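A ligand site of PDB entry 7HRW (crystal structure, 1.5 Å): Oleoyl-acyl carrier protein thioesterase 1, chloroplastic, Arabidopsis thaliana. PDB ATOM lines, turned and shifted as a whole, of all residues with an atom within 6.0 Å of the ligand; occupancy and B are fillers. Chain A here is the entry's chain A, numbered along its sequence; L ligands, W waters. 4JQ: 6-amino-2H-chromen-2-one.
The side-chain hydroxyl (OG1) of Thr 101 is in hydrogen-bond range of a nitrogen (N) of the ligand (2.9 Å). An oxygen (O1) of the ligand sits at hydrogen-bond distance from the guanidinium group of Arg 103 (3.1 Å). A nitrogen (N) of the ligand is in hydrogen-bond range of the side-chain hydroxyl (OG) of Ser 95 (3.3 Å).
O of Gln 94 sits at hydrogen-bond distance from OG1 of Thr 101 (3.3 Å). The guanidinium group (NH1) of Arg 103 is in hydrogen-bond range of the side-chain sulfur (SG) of Cys 93, 3.2 Å away. NH2 of Arg 103 sits at hydrogen-bond distance from ND1 of His 44 (2.9 Å). O of Ala 45 sits at hydrogen-bond distance from N of Phe 50 (3.0 Å). O of Tyr 144 is in hydrogen-bond range of SG of Cys 148 (3.5 Å). NE1 of Trp 68 sits at hydrogen-bond distance from OH of Tyr 144, at 3.0 Å. The backbone carbonyl oxygen of Ala 56 is in hydrogen-bond range of the side-chain hydroxyl of Tyr 144, 2.6 Å away. The backbone carbonyl oxygen (O) of Cys 93 lies close to the side-chain sulfur (SG) of Cys 148, 3.2 Å away.
Residues that only touch the ligand: Ala 45, Tyr 144, Cys 93, Cys 148, Trp 68, His 44, Phe 50 and Ala 56. Hydrophobic or aromatic side chains within 4 Å of the ligand: His 44, Ala 45, Phe 50, Ala 56 and Tyr 144. Of the 19 residues printed, 11 come within 4 Å of the ligand. The nearest printed residue that does not touch the ligand is Phe 147 (4.1 Å).
Water W1 lies within hydrogen-bond range of the side-chain hydroxyl of Ser 95 and a nitrogen (N) of the ligand.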
ATOM      1  N   GLY A  41       0.589  -9.589  22.008  1.00  0.00           N
ATOM      2  CA  GLY A  41      -0.296 -10.683  21.621  1.00  0.00           C
ATOM      3  C   GLY A  41      -1.635 -10.168  21.096  1.00  0.00           C
ATOM      4  O   GLY A  41      -2.149 -10.690  20.093  1.00  0.00           O
ATOM      5  N   HIS A  44      -1.143  -8.594  17.646  1.00  0.00           N
ATOM      6  CA  HIS A  44      -0.981  -9.665  16.656  1.00  0.00           C
ATOM      7  C   HIS A  44      -2.371 -10.205  16.261  1.00  0.00           C
ATOM      8  O   HIS A  44      -2.704 -10.252  15.071  1.00  0.00           O
ATOM      9  CB  HIS A  44      -0.122 -10.818  17.220  1.00  0.00           C
ATOM     10  CG  HIS A  44       0.154 -11.927  16.254  1.00  0.00           C
ATOM     11  ND1 HIS A  44       0.610 -13.175  16.702  1.00  0.00           N
ATOM     12  CD2 HIS A  44      -0.002 -11.970  14.903  1.00  0.00           C
ATOM     13  CE1 HIS A  44       0.777 -13.894  15.593  1.00  0.00           C
ATOM     14  NE2 HIS A  44       0.410 -13.202  14.486  1.00  0.00           N
ATOM     15  N   ALA A  45      -3.230 -10.551  17.254  1.00  0.00           N
ATOM     16  CA  ALA A  45      -4.562 -11.082  16.935  1.00  0.00           C
ATOM     17  C   ALA A  45      -5.381 -10.055  16.107  1.00  0.00           C
ATOM     18  O   ALA A  45      -6.035 -10.419  15.130  1.00  0.00           O
ATOM     19  CB  ALA A  45      -5.334 -11.435  18.218  1.00  0.00           C
ATOM     20  N   GLN A  46      -5.278  -8.756  16.458  1.00  0.00           N
ATOM     21  CA  GLN A  46      -5.999  -7.731  15.709  1.00  0.00           C
ATOM     22  C   GLN A  46      -5.562  -7.693  14.239  1.00  0.00           C
ATOM     23  O   GLN A  46      -6.375  -7.573  13.329  1.00  0.00           O
ATOM     24  CB  GLN A  46      -5.796  -6.335  16.337  1.00  0.00           C
ATOM     25  CG  GLN A  46      -6.692  -5.240  15.704  1.00  0.00           C
ATOM     26  CD  GLN A  46      -6.162  -4.635  14.424  1.00  0.00           C
ATOM     27  OE1 GLN A  46      -4.953  -4.670  14.140  1.00  0.00           O
ATOM     28  NE2 GLN A  46      -7.065  -4.103  13.598  1.00  0.00           N
ATOM     29  N   VAL A  48      -4.502  -9.913  12.244  1.00  0.00           N
ATOM     30  CA  VAL A  48      -4.911 -11.013  11.361  1.00  0.00           C
ATOM     31  C   VAL A  48      -6.428 -11.332  11.432  1.00  0.00           C
ATOM     32  O   VAL A  48      -6.874 -12.308  10.820  1.00  0.00           O
ATOM     33  CB  VAL A  48      -4.029 -12.272  11.573  1.00  0.00           C
ATOM     34  CG1 VAL A  48      -2.571 -11.995  11.181  1.00  0.00           C
ATOM     35  CG2 VAL A  48      -4.102 -12.749  13.026  1.00  0.00           C
ATOM     36  N   PHE A  50      -8.554 -11.795  14.289  1.00  0.00           N
ATOM     37  CA  PHE A  50      -9.167 -12.504  15.424  1.00  0.00           C
ATOM     38  C   PHE A  50      -9.689 -11.482  16.461  1.00  0.00           C
ATOM     39  O   PHE A  50      -9.451 -10.276  16.316  1.00  0.00           O
ATOM     40  CB  PHE A  50      -8.218 -13.564  16.018  1.00  0.00           C
ATOM     41  CG  PHE A  50      -7.789 -14.595  14.998  1.00  0.00           C
ATOM     42  CD1 PHE A  50      -8.724 -15.376  14.335  1.00  0.00           C
ATOM     43  CD2 PHE A  50      -6.458 -14.822  14.723  1.00  0.00           C
ATOM     44  CE1 PHE A  50      -8.342 -16.293  13.361  1.00  0.00           C
ATOM     45  CE2 PHE A  50      -6.074 -15.749  13.747  1.00  0.00           C
ATOM     46  CZ  PHE A  50      -7.013 -16.451  13.063  1.00  0.00           C
ATOM     47  N   PHE A  55      -8.729 -13.169  24.020  1.00  0.00           N
ATOM     48  CA  PHE A  55      -9.079 -14.555  23.739  1.00  0.00           C
ATOM     49  C   PHE A  55      -8.725 -15.002  22.315  1.00  0.00           C
ATOM     50  O   PHE A  55      -8.752 -16.206  22.054  1.00  0.00           O
ATOM     51  CB  PHE A  55     -10.554 -14.840  24.016  1.00  0.00           C
ATOM     52  CG  PHE A  55     -11.066 -14.377  25.366  1.00  0.00           C
ATOM     53  CD1 PHE A  55     -10.438 -14.775  26.535  1.00  0.00           C
ATOM     54  CD2 PHE A  55     -12.224 -13.630  25.474  1.00  0.00           C
ATOM     55  CE1 PHE A  55     -10.927 -14.385  27.778  1.00  0.00           C
ATOM     56  CE2 PHE A  55     -12.708 -13.228  26.717  1.00  0.00           C
ATOM     57  CZ  PHE A  55     -12.061 -13.613  27.858  1.00  0.00           C
ATOM     58  N   ALA A  56      -8.477 -14.053  21.387  1.00  0.00           N
ATOM     59  CA  ALA A  56      -8.094 -14.370  19.991  1.00  0.00           C
ATOM     60  C   ALA A  56      -8.936 -15.471  19.344  1.00  0.00           C
ATOM     61  O   ALA A  56      -8.410 -16.465  18.834  1.00  0.00           O
ATOM     62  CB  ALA A  56      -6.606 -14.714  19.930  1.00  0.00           C
ATOM     63  N   TRP A  68     -10.101 -19.008  24.289  1.00  0.00           N
ATOM     64  CA  TRP A  68      -8.804 -19.532  24.721  1.00  0.00           C
ATOM     65  C   TRP A  68      -8.512 -18.932  26.090  1.00  0.00           C
ATOM     66  O   TRP A  68      -8.707 -17.719  26.281  1.00  0.00           O
ATOM     67  CB  TRP A  68      -7.694 -19.038  23.762  1.00  0.00           C
ATOM     68  CG  TRP A  68      -7.723 -19.672  22.398  1.00  0.00           C
ATOM     69  CD1 TRP A  68      -7.977 -19.056  21.210  1.00  0.00           C
ATOM     70  CD2 TRP A  68      -7.391 -21.039  22.084  1.00  0.00           C
ATOM     71  NE1 TRP A  68      -7.844 -19.952  20.169  1.00  0.00           N
ATOM     72  CE2 TRP A  68      -7.508 -21.175  20.682  1.00  0.00           C
ATOM     73  CE3 TRP A  68      -7.076 -22.172  22.847  1.00  0.00           C
ATOM     74  CZ2 TRP A  68      -7.214 -22.382  20.033  1.00  0.00           C
ATOM     75  CZ3 TRP A  68      -6.809 -23.365  22.201  1.00  0.00           C
ATOM     76  CH2 TRP A  68      -6.912 -23.468  20.809  1.00  0.00           C
ATOM     77  N   CYS A  93       2.304 -17.762  17.269  1.00  0.00           N
ATOM     78  CA  CYS A  93       1.569 -18.875  17.877  1.00  0.00           C
ATOM     79  C   CYS A  93       1.879 -20.144  17.115  1.00  0.00           C
ATOM     80  O   CYS A  93       2.206 -20.103  15.933  1.00  0.00           O
ATOM     81  CB  CYS A  93       0.066 -18.631  17.855  1.00  0.00           C
ATOM     82  SG  CYS A  93      -0.492 -17.218  18.828  1.00  0.00           S
ATOM     83  N   GLN A  94       1.581 -21.287  17.742  1.00  0.00           N
ATOM     84  CA  GLN A  94       1.651 -22.583  17.067  1.00  0.00           C
ATOM     85  C   GLN A  94       0.675 -23.517  17.757  1.00  0.00           C
ATOM     86  O   GLN A  94       0.729 -23.654  18.984  1.00  0.00           O
ATOM     87  CB  GLN A  94       3.070 -23.161  17.134  1.00  0.00           C
ATOM     88  CG  GLN A  94       3.945 -22.804  15.950  1.00  0.00           C
ATOM     89  CD  GLN A  94       4.960 -23.882  15.638  1.00  0.00           C
ATOM     90  OE1 GLN A  94       5.716 -24.331  16.516  1.00  0.00           O
ATOM     91  NE2 GLN A  94       5.036 -24.253  14.364  1.00  0.00           N
ATOM     92  N   SER A  95      -0.219 -24.175  16.994  1.00  0.00           N
ATOM     93  CA  SER A  95      -1.154 -25.118  17.600  1.00  0.00           C
ATOM     94  C   SER A  95      -0.411 -26.325  18.162  1.00  0.00           C
ATOM     95  O   SER A  95       0.668 -26.690  17.647  1.00  0.00           O
ATOM     96  CB  SER A  95      -2.175 -25.606  16.576  1.00  0.00           C
ATOM     97  OG  SER A  95      -2.908 -24.513  16.048  1.00  0.00           O
ATOM     98  N   GLY A 100      -4.294 -27.960  22.870  1.00  0.00           N
ATOM     99  CA  GLY A 100      -4.470 -26.512  22.954  1.00  0.00           C
ATOM    100  C   GLY A 100      -3.543 -25.794  22.005  1.00  0.00           C
ATOM    101  O   GLY A 100      -3.238 -26.319  20.919  1.00  0.00           O
ATOM    102  N   THR A 101      -3.092 -24.616  22.378  1.00  0.00           N
ATOM    103  CA  THR A 101      -2.198 -23.843  21.516  1.00  0.00           C
ATOM    104  C   THR A 101      -1.124 -23.142  22.350  1.00  0.00           C
ATOM    105  O   THR A 101      -1.204 -23.103  23.581  1.00  0.00           O
ATOM    106  CB  THR A 101      -3.035 -22.871  20.677  1.00  0.00           C
ATOM    107  OG1 THR A 101      -2.214 -22.352  19.635  1.00  0.00           O
ATOM    108  CG2 THR A 101      -3.602 -21.730  21.530  1.00  0.00           C
ATOM    109  N   ARG A 102      -0.109 -22.629  21.674  1.00  0.00           N
ATOM    110  CA  ARG A 102       1.018 -22.012  22.354  1.00  0.00           C
ATOM    111  C   ARG A 102       1.280 -20.629  21.753  1.00  0.00           C
ATOM    112  O   ARG A 102       1.215 -20.486  20.531  1.00  0.00           O
ATOM    113  CB  ARG A 102       2.255 -22.893  22.107  1.00  0.00           C
ATOM    114  CG  ARG A 102       3.460 -22.584  22.987  1.00  0.00           C
ATOM    115  CD  ARG A 102       4.610 -23.542  22.733  1.00  0.00           C
ATOM    116  NE  ARG A 102       5.401 -23.110  21.583  1.00  0.00           N
ATOM    117  CZ  ARG A 102       5.364 -23.658  20.376  1.00  0.00           C
ATOM    118  NH1 ARG A 102       6.075 -23.152  19.390  1.00  0.00           N
ATOM    119  NH2 ARG A 102       4.626 -24.733  20.159  1.00  0.00           N
ATOM    120  N   ARG A 103       1.564 -19.620  22.601  1.00  0.00           N
ATOM    121  CA  ARG A 103       2.017 -18.329  22.115  1.00  0.00           C
ATOM    122  C   ARG A 103       3.377 -18.145  22.737  1.00  0.00           C
ATOM    123  O   ARG A 103       3.511 -18.219  23.971  1.00  0.00           O
ATOM    124  CB  ARG A 103       1.121 -17.123  22.514  1.00  0.00           C
ATOM    125  CG  ARG A 103       1.744 -15.797  22.037  1.00  0.00           C
ATOM    126  CD  ARG A 103       0.807 -14.599  22.255  1.00  0.00           C
ATOM    127  NE  ARG A 103      -0.352 -14.601  21.354  1.00  0.00           N
ATOM    128  CZ  ARG A 103      -0.317 -14.203  20.081  1.00  0.00           C
ATOM    129  NH1 ARG A 103      -1.425 -14.211  19.344  1.00  0.00           N
ATOM    130  NH2 ARG A 103       0.821 -13.787  19.548  1.00  0.00           N
ATOM    131  N   TYR A 144      -6.616 -21.829  12.102  1.00  0.00           N
ATOM    132  CA  TYR A 144      -5.442 -21.063  12.542  1.00  0.00           C
ATOM    133  C   TYR A 144      -4.134 -21.429  11.821  1.00  0.00           C
ATOM    134  O   TYR A 144      -3.160 -20.669  11.896  1.00  0.00           O
ATOM    135  CB  TYR A 144      -5.214 -21.314  14.031  1.00  0.00           C
ATOM    136  CG  TYR A 144      -6.220 -20.632  14.941  1.00  0.00           C
ATOM    137  CD1 TYR A 144      -6.233 -19.245  15.068  1.00  0.00           C
ATOM    138  CD2 TYR A 144      -7.082 -21.369  15.741  1.00  0.00           C
ATOM    139  CE1 TYR A 144      -7.106 -18.614  15.949  1.00  0.00           C
ATOM    140  CE2 TYR A 144      -7.950 -20.749  16.628  1.00  0.00           C
ATOM    141  CZ  TYR A 144      -7.935 -19.375  16.753  1.00  0.00           C
ATOM    142  OH  TYR A 144      -8.800 -18.764  17.637  1.00  0.00           O
ATOM    143  N   PHE A 147      -1.915 -18.889   9.862  1.00  0.00           N
ATOM    144  CA  PHE A 147      -1.394 -17.743  10.607  1.00  0.00           C
ATOM    145  C   PHE A 147      -0.173 -18.127  11.495  1.00  0.00           C
ATOM    146  O   PHE A 147       0.340 -17.269  12.226  1.00  0.00           O
ATOM    147  CB  PHE A 147      -2.509 -17.175  11.504  1.00  0.00           C
ATOM    148  CG  PHE A 147      -3.671 -16.707  10.646  1.00  0.00           C
ATOM    149  CD1 PHE A 147      -3.574 -15.538   9.900  1.00  0.00           C
ATOM    150  CD2 PHE A 147      -4.807 -17.478  10.518  1.00  0.00           C
ATOM    151  CE1 PHE A 147      -4.622 -15.132   9.073  1.00  0.00           C
ATOM    152  CE2 PHE A 147      -5.845 -17.086   9.674  1.00  0.00           C
ATOM    153  CZ  PHE A 147      -5.761 -15.891   8.981  1.00  0.00           C
ATOM    154  N   CYS A 148       0.259 -19.397  11.458  1.00  0.00           N
ATOM    155  CA  CYS A 148       1.371 -19.916  12.253  1.00  0.00           C
ATOM    156  C   CYS A 148       2.479 -20.456  11.363  1.00  0.00           C
ATOM    157  O   CYS A 148       2.184 -21.012  10.274  1.00  0.00           O
ATOM    158  CB  CYS A 148       0.854 -21.019  13.152  1.00  0.00           C
ATOM    159  SG  CYS A 148      -0.506 -20.523  14.231  1.00  0.00           S
HETATM  160  C1  4JQ L   1      -4.646 -19.587  18.301  1.00  0.00           C
HETATM  161  C2  4JQ L   1      -4.676 -18.213  18.336  1.00  0.00           C
HETATM  162  C3  4JQ L   1      -3.899 -17.497  17.438  1.00  0.00           C
HETATM  163  C4  4JQ L   1      -3.179 -15.332  16.673  1.00  0.00           C
HETATM  164  C5  4JQ L   1      -2.402 -15.977  15.700  1.00  0.00           C
HETATM  165  C6  4JQ L   1      -2.390 -17.316  15.590  1.00  0.00           C
HETATM  166  C7  4JQ L   1      -3.121 -18.134  16.477  1.00  0.00           C
HETATM  167  C8  4JQ L   1      -3.103 -19.556  16.452  1.00  0.00           C
HETATM  168  O1  4JQ L   1      -3.240 -14.137  16.871  1.00  0.00           O
HETATM  169  O   4JQ L   1      -4.004 -16.120  17.461  1.00  0.00           O
HETATM  170  C   4JQ L   1      -3.858 -20.290  17.360  1.00  0.00           C
HETATM  171  N   4JQ L   1      -3.868 -21.682  17.350  1.00  0.00           N
HETATM  172  O   HOH W   1      -5.549 -24.365  17.193  1.00  0.00           O
